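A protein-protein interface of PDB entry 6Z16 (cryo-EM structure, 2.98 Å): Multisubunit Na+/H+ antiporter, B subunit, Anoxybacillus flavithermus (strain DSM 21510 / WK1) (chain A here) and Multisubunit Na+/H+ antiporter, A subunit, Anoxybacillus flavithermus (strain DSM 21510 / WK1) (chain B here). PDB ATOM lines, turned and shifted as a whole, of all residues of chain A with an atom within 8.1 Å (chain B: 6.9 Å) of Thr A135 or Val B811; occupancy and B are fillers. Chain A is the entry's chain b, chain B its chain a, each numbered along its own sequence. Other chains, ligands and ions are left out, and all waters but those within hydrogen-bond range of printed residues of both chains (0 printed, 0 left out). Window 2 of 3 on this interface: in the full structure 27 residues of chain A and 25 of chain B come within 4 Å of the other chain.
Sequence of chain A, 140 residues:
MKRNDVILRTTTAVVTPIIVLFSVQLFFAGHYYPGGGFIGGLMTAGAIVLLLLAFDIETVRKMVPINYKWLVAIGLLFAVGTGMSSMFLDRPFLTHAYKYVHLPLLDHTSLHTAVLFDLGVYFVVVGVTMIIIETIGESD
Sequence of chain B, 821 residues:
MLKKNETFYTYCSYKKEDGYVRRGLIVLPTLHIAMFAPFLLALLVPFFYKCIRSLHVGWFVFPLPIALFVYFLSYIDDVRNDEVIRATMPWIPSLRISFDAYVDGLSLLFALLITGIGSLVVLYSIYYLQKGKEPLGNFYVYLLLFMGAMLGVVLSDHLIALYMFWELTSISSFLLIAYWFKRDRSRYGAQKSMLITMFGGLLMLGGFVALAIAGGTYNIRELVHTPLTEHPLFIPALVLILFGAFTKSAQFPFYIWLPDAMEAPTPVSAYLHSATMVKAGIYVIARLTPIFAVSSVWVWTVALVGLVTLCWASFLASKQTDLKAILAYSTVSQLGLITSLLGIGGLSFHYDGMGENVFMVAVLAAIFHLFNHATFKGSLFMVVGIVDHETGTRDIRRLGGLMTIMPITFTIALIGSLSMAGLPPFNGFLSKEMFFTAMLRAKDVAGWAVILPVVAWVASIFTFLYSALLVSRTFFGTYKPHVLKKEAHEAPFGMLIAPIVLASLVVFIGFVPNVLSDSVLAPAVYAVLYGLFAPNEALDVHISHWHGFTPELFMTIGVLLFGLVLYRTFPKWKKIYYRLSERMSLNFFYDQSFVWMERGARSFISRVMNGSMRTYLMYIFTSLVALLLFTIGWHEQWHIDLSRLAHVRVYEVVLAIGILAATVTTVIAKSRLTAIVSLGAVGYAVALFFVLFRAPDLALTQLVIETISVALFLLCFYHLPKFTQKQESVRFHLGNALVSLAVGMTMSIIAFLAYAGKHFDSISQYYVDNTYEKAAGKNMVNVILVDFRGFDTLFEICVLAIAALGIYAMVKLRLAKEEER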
ATOM      1  N   LEU A  52     -11.117 -25.452 -28.409  1.00  0.00           N
ATOM      2  CA  LEU A  52     -10.328 -25.019 -27.256  1.00  0.00           C
ATOM      3  C   LEU A  52      -9.100 -25.889 -27.049  1.00  0.00           C
ATOM      4  O   LEU A  52      -8.065 -25.402 -26.586  1.00  0.00           O
ATOM      5  CB  LEU A  52     -11.172 -25.049 -25.983  1.00  0.00           C
ATOM      6  CG  LEU A  52     -12.253 -24.002 -25.773  1.00  0.00           C
ATOM      7  CD1 LEU A  52     -13.097 -24.383 -24.586  1.00  0.00           C
ATOM      8  CD2 LEU A  52     -11.593 -22.674 -25.535  1.00  0.00           C
ATOM      9  N   ILE A  57      -7.162 -19.817 -25.382  1.00  0.00           N
ATOM     10  CA  ILE A  57      -8.427 -19.451 -24.755  1.00  0.00           C
ATOM     11  C   ILE A  57      -8.888 -18.111 -25.321  1.00  0.00           C
ATOM     12  O   ILE A  57     -10.090 -17.843 -25.410  1.00  0.00           O
ATOM     13  CB  ILE A  57      -8.304 -19.435 -23.213  1.00  0.00           C
ATOM     14  CG1 ILE A  57      -9.667 -19.255 -22.535  1.00  0.00           C
ATOM     15  CG2 ILE A  57      -7.283 -18.405 -22.719  1.00  0.00           C
ATOM     16  CD1 ILE A  57     -10.603 -20.410 -22.726  1.00  0.00           C
ATOM     17  N   ARG A  61     -12.327 -17.424 -28.347  1.00  0.00           N
ATOM     18  CA  ARG A  61     -13.288 -16.334 -28.239  1.00  0.00           C
ATOM     19  C   ARG A  61     -13.067 -15.271 -29.306  1.00  0.00           C
ATOM     20  O   ARG A  61     -13.967 -14.462 -29.548  1.00  0.00           O
ATOM     21  CB  ARG A  61     -13.254 -15.685 -26.854  1.00  0.00           C
ATOM     22  CG  ARG A  61     -11.967 -14.972 -26.503  1.00  0.00           C
ATOM     23  CD  ARG A  61     -12.151 -14.120 -25.257  1.00  0.00           C
ATOM     24  NE  ARG A  61     -12.513 -14.894 -24.075  1.00  0.00           N
ATOM     25  CZ  ARG A  61     -11.640 -15.359 -23.191  1.00  0.00           C
ATOM     26  NH1 ARG A  61     -10.346 -15.119 -23.347  1.00  0.00           N
ATOM     27  NH2 ARG A  61     -12.065 -16.051 -22.144  1.00  0.00           N
ATOM     28  N   LYS A  69     -22.901 -15.821 -20.997  1.00  0.00           N
ATOM     29  CA  LYS A  69     -23.864 -15.387 -19.997  1.00  0.00           C
ATOM     30  C   LYS A  69     -25.074 -14.740 -20.660  1.00  0.00           C
ATOM     31  O   LYS A  69     -26.225 -14.968 -20.249  1.00  0.00           O
ATOM     32  CB  LYS A  69     -23.159 -14.443 -19.027  1.00  0.00           C
ATOM     33  CG  LYS A  69     -22.039 -15.162 -18.283  1.00  0.00           C
ATOM     34  CD  LYS A  69     -21.303 -14.314 -17.275  1.00  0.00           C
ATOM     35  CE  LYS A  69     -19.953 -13.843 -17.782  1.00  0.00           C
ATOM     36  NZ  LYS A  69     -20.052 -12.751 -18.779  1.00  0.00           N
ATOM     37  N   GLY A 127     -24.330 -22.345 -23.396  1.00  0.00           N
ATOM     38  CA  GLY A 127     -23.759 -21.300 -22.568  1.00  0.00           C
ATOM     39  C   GLY A 127     -23.238 -21.796 -21.234  1.00  0.00           C
ATOM     40  O   GLY A 127     -22.148 -21.412 -20.821  1.00  0.00           O
ATOM     41  N   VAL A 128     -23.989 -22.678 -20.563  1.00  0.00           N
ATOM     42  CA  VAL A 128     -23.587 -23.202 -19.257  1.00  0.00           C
ATOM     43  C   VAL A 128     -22.314 -24.030 -19.373  1.00  0.00           C
ATOM     44  O   VAL A 128     -21.369 -23.855 -18.586  1.00  0.00           O
ATOM     45  CB  VAL A 128     -24.740 -24.011 -18.631  1.00  0.00           C
ATOM     46  CG1 VAL A 128     -24.249 -24.881 -17.496  1.00  0.00           C
ATOM     47  CG2 VAL A 128     -25.794 -23.073 -18.088  1.00  0.00           C
ATOM     48  N   THR A 129     -22.257 -24.919 -20.377  1.00  0.00           N
ATOM     49  CA  THR A 129     -21.078 -25.761 -20.555  1.00  0.00           C
ATOM     50  C   THR A 129     -19.845 -24.928 -20.886  1.00  0.00           C
ATOM     51  O   THR A 129     -18.764 -25.145 -20.314  1.00  0.00           O
ATOM     52  CB  THR A 129     -21.341 -26.790 -21.649  1.00  0.00           C
ATOM     53  OG1 THR A 129     -22.515 -27.537 -21.321  1.00  0.00           O
ATOM     54  CG2 THR A 129     -20.194 -27.752 -21.743  1.00  0.00           C
ATOM     55  N   MET A 130     -20.008 -23.914 -21.740  1.00  0.00           N
ATOM     56  CA  MET A 130     -18.860 -23.080 -22.063  1.00  0.00           C
ATOM     57  C   MET A 130     -18.441 -22.179 -20.909  1.00  0.00           C
ATOM     58  O   MET A 130     -17.241 -21.946 -20.746  1.00  0.00           O
ATOM     59  CB  MET A 130     -19.135 -22.261 -23.316  1.00  0.00           C
ATOM     60  CG  MET A 130     -19.089 -23.088 -24.583  1.00  0.00           C
ATOM     61  SD  MET A 130     -17.509 -23.949 -24.695  1.00  0.00           S
ATOM     62  CE  MET A 130     -16.373 -22.567 -24.776  1.00  0.00           C
ATOM     63  N   ILE A 131     -19.391 -21.697 -20.092  1.00  0.00           N
ATOM     64  CA  ILE A 131     -19.048 -20.900 -18.909  1.00  0.00           C
ATOM     65  C   ILE A 131     -18.218 -21.721 -17.935  1.00  0.00           C
ATOM     66  O   ILE A 131     -17.173 -21.262 -17.463  1.00  0.00           O
ATOM     67  CB  ILE A 131     -20.316 -20.346 -18.227  1.00  0.00           C
ATOM     68  CG1 ILE A 131     -20.898 -19.163 -18.983  1.00  0.00           C
ATOM     69  CG2 ILE A 131     -20.028 -19.880 -16.812  1.00  0.00           C
ATOM     70  CD1 ILE A 131     -22.307 -18.850 -18.544  1.00  0.00           C
ATOM     71  N   ILE A 132     -18.652 -22.962 -17.668  1.00  0.00           N
ATOM     72  CA  ILE A 132     -17.928 -23.850 -16.752  1.00  0.00           C
ATOM     73  C   ILE A 132     -16.510 -24.102 -17.247  1.00  0.00           C
ATOM     74  O   ILE A 132     -15.532 -23.905 -16.511  1.00  0.00           O
ATOM     75  CB  ILE A 132     -18.694 -25.171 -16.566  1.00  0.00           C
ATOM     76  CG1 ILE A 132     -19.997 -24.941 -15.800  1.00  0.00           C
ATOM     77  CG2 ILE A 132     -17.835 -26.199 -15.868  1.00  0.00           C
ATOM     78  CD1 ILE A 132     -20.905 -26.143 -15.771  1.00  0.00           C
ATOM     79  N   ILE A 133     -16.372 -24.451 -18.526  1.00  0.00           N
ATOM     80  CA  ILE A 133     -15.073 -24.884 -19.031  1.00  0.00           C
ATOM     81  C   ILE A 133     -14.107 -23.708 -19.175  1.00  0.00           C
ATOM     82  O   ILE A 133     -12.953 -23.786 -18.734  1.00  0.00           O
ATOM     83  CB  ILE A 133     -15.262 -25.668 -20.337  1.00  0.00           C
ATOM     84  CG1 ILE A 133     -15.985 -26.970 -19.996  1.00  0.00           C
ATOM     85  CG2 ILE A 133     -13.934 -25.932 -21.013  1.00  0.00           C
ATOM     86  CD1 ILE A 133     -16.523 -27.704 -21.145  1.00  0.00           C
ATOM     87  N   GLU A 134     -14.557 -22.585 -19.741  1.00  0.00           N
ATOM     88  CA  GLU A 134     -13.605 -21.487 -19.857  1.00  0.00           C
ATOM     89  C   GLU A 134     -13.481 -20.672 -18.578  1.00  0.00           C
ATOM     90  O   GLU A 134     -12.624 -19.789 -18.522  1.00  0.00           O
ATOM     91  CB  GLU A 134     -13.951 -20.552 -21.019  1.00  0.00           C
ATOM     92  CG  GLU A 134     -15.089 -19.581 -20.772  1.00  0.00           C
ATOM     93  CD  GLU A 134     -15.415 -18.751 -22.001  1.00  0.00           C
ATOM     94  OE1 GLU A 134     -14.734 -18.931 -23.033  1.00  0.00           O
ATOM     95  OE2 GLU A 134     -16.357 -17.933 -21.944  1.00  0.00           O
ATOM     96  N   THR A 135     -14.299 -20.937 -17.554  1.00  0.00           N
ATOM     97  CA  THR A 135     -14.060 -20.347 -16.245  1.00  0.00           C
ATOM     98  C   THR A 135     -13.000 -21.132 -15.491  1.00  0.00           C
ATOM     99  O   THR A 135     -12.109 -20.545 -14.866  1.00  0.00           O
ATOM    100  CB  THR A 135     -15.366 -20.306 -15.447  1.00  0.00           C
ATOM    101  OG1 THR A 135     -16.342 -19.550 -16.170  1.00  0.00           O
ATOM    102  CG2 THR A 135     -15.159 -19.665 -14.088  1.00  0.00           C
ATOM    103  N   ILE A 136     -13.082 -22.462 -15.559  1.00  0.00           N
ATOM    104  CA  ILE A 136     -12.068 -23.316 -14.955  1.00  0.00           C
ATOM    105  C   ILE A 136     -10.721 -23.160 -15.658  1.00  0.00           C
ATOM    106  O   ILE A 136      -9.671 -23.166 -15.002  1.00  0.00           O
ATOM    107  CB  ILE A 136     -12.588 -24.766 -14.962  1.00  0.00           C
ATOM    108  CG1 ILE A 136     -13.743 -24.905 -13.973  1.00  0.00           C
ATOM    109  CG2 ILE A 136     -11.510 -25.759 -14.644  1.00  0.00           C
ATOM    110  CD1 ILE A 136     -14.475 -26.195 -14.095  1.00  0.00           C
ATOM    111  N   GLY A 137     -10.729 -22.938 -16.976  1.00  0.00           N
ATOM    112  CA  GLY A 137      -9.483 -22.931 -17.731  1.00  0.00           C
ATOM    113  C   GLY A 137      -8.569 -21.757 -17.429  1.00  0.00           C
ATOM    114  O   GLY A 137      -7.351 -21.923 -17.324  1.00  0.00           O
ATOM    115  N   GLU A 138      -9.132 -20.561 -17.278  1.00  0.00           N
ATOM    116  CA  GLU A 138      -8.335 -19.359 -17.069  1.00  0.00           C
ATOM    117  C   GLU A 138      -8.250 -18.959 -15.600  1.00  0.00           C
ATOM    118  O   GLU A 138      -7.923 -17.807 -15.294  1.00  0.00           O
ATOM    119  CB  GLU A 138      -8.894 -18.211 -17.910  1.00  0.00           C
ATOM    120  CG  GLU A 138     -10.302 -17.788 -17.536  1.00  0.00           C
ATOM    121  CD  GLU A 138     -10.889 -16.784 -18.508  1.00  0.00           C
ATOM    122  OE1 GLU A 138     -10.190 -16.400 -19.468  1.00  0.00           O
ATOM    123  OE2 GLU A 138     -12.056 -16.387 -18.321  1.00  0.00           O
ATOM    124  N   SER A 139      -8.508 -19.897 -14.688  1.00  0.00           N
ATOM    125  CA  SER A 139      -8.526 -19.577 -13.264  1.00  0.00           C
ATOM    126  C   SER A 139      -7.119 -19.334 -12.727  1.00  0.00           C
ATOM    127  O   SER A 139      -6.859 -18.297 -12.102  1.00  0.00           O
ATOM    128  CB  SER A 139      -9.208 -20.704 -12.492  1.00  0.00           C
ATOM    129  OG  SER A 139      -9.196 -20.452 -11.101  1.00  0.00           O
ATOM    130  N   ASP A 140      -6.208 -20.281 -12.971  1.00  0.00           N
ATOM    131  CA  ASP A 140      -4.813 -20.291 -12.494  1.00  0.00           C
ATOM    132  C   ASP A 140      -4.727 -20.125 -10.972  1.00  0.00           C
ATOM    133  O   ASP A 140      -4.002 -20.857 -10.297  1.00  0.00           O
ATOM    134  CB  ASP A 140      -3.984 -19.206 -13.202  1.00  0.00           C
ATOM    135  CG  ASP A 140      -2.480 -19.419 -13.064  1.00  0.00           C
ATOM    136  OD1 ASP A 140      -2.050 -20.424 -12.457  1.00  0.00           O
ATOM    137  OD2 ASP A 140      -1.718 -18.568 -13.567  1.00  0.00           O
ATOM    138  N   ALA B 804     -23.959 -22.590 -13.306  1.00  0.00           N
ATOM    139  CA  ALA B 804     -22.897 -21.938 -14.074  1.00  0.00           C
ATOM    140  C   ALA B 804     -22.531 -20.577 -13.493  1.00  0.00           C
ATOM    141  O   ALA B 804     -21.340 -20.246 -13.370  1.00  0.00           O
ATOM    142  CB  ALA B 804     -23.319 -21.792 -15.531  1.00  0.00           C
ATOM    143  N   GLY B 806     -22.921 -19.672 -10.401  1.00  0.00           N
ATOM    144  CA  GLY B 806     -22.273 -19.890  -9.124  1.00  0.00           C
ATOM    145  C   GLY B 806     -20.832 -20.330  -9.257  1.00  0.00           C
ATOM    146  O   GLY B 806     -19.986 -19.931  -8.458  1.00  0.00           O
ATOM    147  N   ILE B 807     -20.536 -21.168 -10.257  1.00  0.00           N
ATOM    148  CA  ILE B 807     -19.151 -21.556 -10.518  1.00  0.00           C
ATOM    149  C   ILE B 807     -18.324 -20.344 -10.931  1.00  0.00           C
ATOM    150  O   ILE B 807     -17.195 -20.150 -10.448  1.00  0.00           O
ATOM    151  CB  ILE B 807     -19.108 -22.682 -11.569  1.00  0.00           C
ATOM    152  CG1 ILE B 807     -19.661 -23.971 -10.975  1.00  0.00           C
ATOM    153  CG2 ILE B 807     -17.706 -22.921 -12.076  1.00  0.00           C
ATOM    154  CD1 ILE B 807     -19.908 -25.035 -11.981  1.00  0.00           C
ATOM    155  N   TYR B 808     -18.900 -19.478 -11.776  1.00  0.00           N
ATOM    156  CA  TYR B 808     -18.225 -18.237 -12.154  1.00  0.00           C
ATOM    157  C   TYR B 808     -17.992 -17.330 -10.948  1.00  0.00           C
ATOM    158  O   TYR B 808     -16.905 -16.756 -10.792  1.00  0.00           O
ATOM    159  CB  TYR B 808     -19.040 -17.505 -13.222  1.00  0.00           C
ATOM    160  CG  TYR B 808     -18.406 -16.220 -13.698  1.00  0.00           C
ATOM    161  CD1 TYR B 808     -17.321 -16.240 -14.565  1.00  0.00           C
ATOM    162  CD2 TYR B 808     -18.888 -14.988 -13.278  1.00  0.00           C
ATOM    163  CE1 TYR B 808     -16.737 -15.069 -15.002  1.00  0.00           C
ATOM    164  CE2 TYR B 808     -18.305 -13.813 -13.704  1.00  0.00           C
ATOM    165  CZ  TYR B 808     -17.230 -13.859 -14.564  1.00  0.00           C
ATOM    166  OH  TYR B 808     -16.652 -12.690 -14.991  1.00  0.00           O
ATOM    167  N   ALA B 809     -18.985 -17.238 -10.058  1.00  0.00           N
ATOM    168  CA  ALA B 809     -18.877 -16.362  -8.897  1.00  0.00           C
ATOM    169  C   ALA B 809     -17.882 -16.895  -7.872  1.00  0.00           C
ATOM    170  O   ALA B 809     -17.186 -16.110  -7.220  1.00  0.00           O
ATOM    171  CB  ALA B 809     -20.252 -16.177  -8.264  1.00  0.00           C
ATOM    172  N   MET B 810     -17.806 -18.220  -7.704  1.00  0.00           N
ATOM    173  CA  MET B 810     -16.831 -18.788  -6.779  1.00  0.00           C
ATOM    174  C   MET B 810     -15.414 -18.615  -7.289  1.00  0.00           C
ATOM    175  O   MET B 810     -14.503 -18.338  -6.503  1.00  0.00           O
ATOM    176  CB  MET B 810     -17.072 -20.275  -6.541  1.00  0.00           C
ATOM    177  CG  MET B 810     -18.302 -20.647  -5.784  1.00  0.00           C
ATOM    178  SD  MET B 810     -18.186 -22.395  -5.392  1.00  0.00           S
ATOM    179  CE  MET B 810     -18.208 -23.103  -7.030  1.00  0.00           C
ATOM    180  N   VAL B 811     -15.197 -18.810  -8.590  1.00  0.00           N
ATOM    181  CA  VAL B 811     -13.835 -18.715  -9.103  1.00  0.00           C
ATOM    182  C   VAL B 811     -13.374 -17.260  -9.145  1.00  0.00           C
ATOM    183  O   VAL B 811     -12.224 -16.952  -8.810  1.00  0.00           O
ATOM    184  CB  VAL B 811     -13.739 -19.413 -10.473  1.00  0.00           C
ATOM    185  CG1 VAL B 811     -12.376 -19.208 -11.106  1.00  0.00           C
ATOM    186  CG2 VAL B 811     -13.996 -20.896 -10.309  1.00  0.00           C
ATOM    187  N   LYS B 812     -14.269 -16.331  -9.483  1.00  0.00           N
ATOM    188  CA  LYS B 812     -13.803 -14.965  -9.710  1.00  0.00           C
ATOM    189  C   LYS B 812     -13.736 -14.100  -8.451  1.00  0.00           C
ATOM    190  O   LYS B 812     -12.855 -13.239  -8.352  1.00  0.00           O
ATOM    191  CB  LYS B 812     -14.680 -14.291 -10.764  1.00  0.00           C
ATOM    192  CG  LYS B 812     -14.584 -14.887 -12.172  1.00  0.00           C
ATOM    193  CD  LYS B 812     -13.289 -14.511 -12.909  1.00  0.00           C
ATOM    194  CE  LYS B 812     -12.251 -15.636 -12.930  1.00  0.00           C
ATOM    195  NZ  LYS B 812     -11.049 -15.289 -13.734  1.00  0.00           N
ATOM    196  N   LEU B 813     -14.635 -14.289  -7.488  1.00  0.00           N
ATOM    197  CA  LEU B 813     -14.709 -13.402  -6.332  1.00  0.00           C
ATOM    198  C   LEU B 813     -13.777 -13.932  -5.248  1.00  0.00           C
ATOM    199  O   LEU B 813     -13.956 -15.057  -4.770  1.00  0.00           O
ATOM    200  CB  LEU B 813     -16.143 -13.319  -5.814  1.00  0.00           C
ATOM    201  CG  LEU B 813     -16.626 -12.087  -5.047  1.00  0.00           C
ATOM    202  CD1 LEU B 813     -18.126 -12.073  -5.068  1.00  0.00           C
ATOM    203  CD2 LEU B 813     -16.150 -12.018  -3.642  1.00  0.00           C
ATOM    204  N   ARG B 814     -12.787 -13.130  -4.860  1.00  0.00           N
ATOM    205  CA  ARG B 814     -11.769 -13.546  -3.893  1.00  0.00           C
ATOM    206  C   ARG B 814     -11.490 -12.442  -2.870  1.00  0.00           C
ATOM    207  O   ARG B 814     -10.345 -12.032  -2.676  1.00  0.00           O
ATOM    208  CB  ARG B 814     -10.480 -13.966  -4.597  1.00  0.00           C
ATOM    209  CG  ARG B 814     -10.587 -15.279  -5.348  1.00  0.00           C
ATOM    210  CD  ARG B 814      -9.296 -15.653  -6.021  1.00  0.00           C
ATOM    211  NE  ARG B 814      -9.443 -16.884  -6.784  1.00  0.00           N
ATOM    212  CZ  ARG B 814      -8.481 -17.420  -7.524  1.00  0.00           C
ATOM    213  NH1 ARG B 814      -7.295 -16.829  -7.600  1.00  0.00           N
ATOM    214  NH2 ARG B 814      -8.704 -18.543  -8.189  1.00  0.00           N
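The guanidinium group (NE) of Arg B814 is in hydrogen-bond range of the backbone carbonyl oxygen (O) of Val B811 (3.4 Å).
Printed residues of chain B that touch a printed residue of chain A: Ala B804, Ile B807, Tyr B808, Val B811 and Arg B814. Of the 18 printed residues of chain A, 5 touch a printed residue of chain B. Printed residues of chain A that touch a printed residue of chain B: Val A128, Ile A131, Ile A132, Thr A135 and Ser A139. Hydrophobic or aromatic side chains of chain A that line the printed part of chain B: Val A128, Ile A131 and Ile A132. Among the printed residues, no Asp or Glu carboxylate lies within 4 Å of a Lys or Arg side-chain nitrogen of the other chain.
Of the printed residues of chain B, Val A128 touches Ala B804 (3.8 Å). Thr A129 touches none of the printed residues of chain B. Printed residues of chain B within 4 Å of Ile A132: Ile B807 (3.8 Å). Thr A135 touches just these residues of chain B: Tyr B808 and Val B811. Of the printed residues of chain B, Ser A139 touches Val B811 and Arg B814. Of the printed residues of chain A, Ala B804 touches Val A128 and Ile A131. Of the printed residues of chain A, Ile B807 touches Ile A132. Of chain A, only Thr A135 and Ser A139 come within 4 Å of Val B811. The nearest residue of chain A that does not touch Val B811 is Ile A136 (5.4 Å).
Among the printed residues, pairs that only touch across the chains: Val A128 with Ala B804 (3.8 Å), Ile A131 with Ala B804 (3.7 Å), Ile A132 with Ile B807 (3.8 Å), Thr A135 with Tyr B808 (3.8 Å), Thr A135 with Val B811 (3.9 Å), Ser A139 with Val B811 (3.4 Å) and Ser A139 with Arg B814 (3.5 Å).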
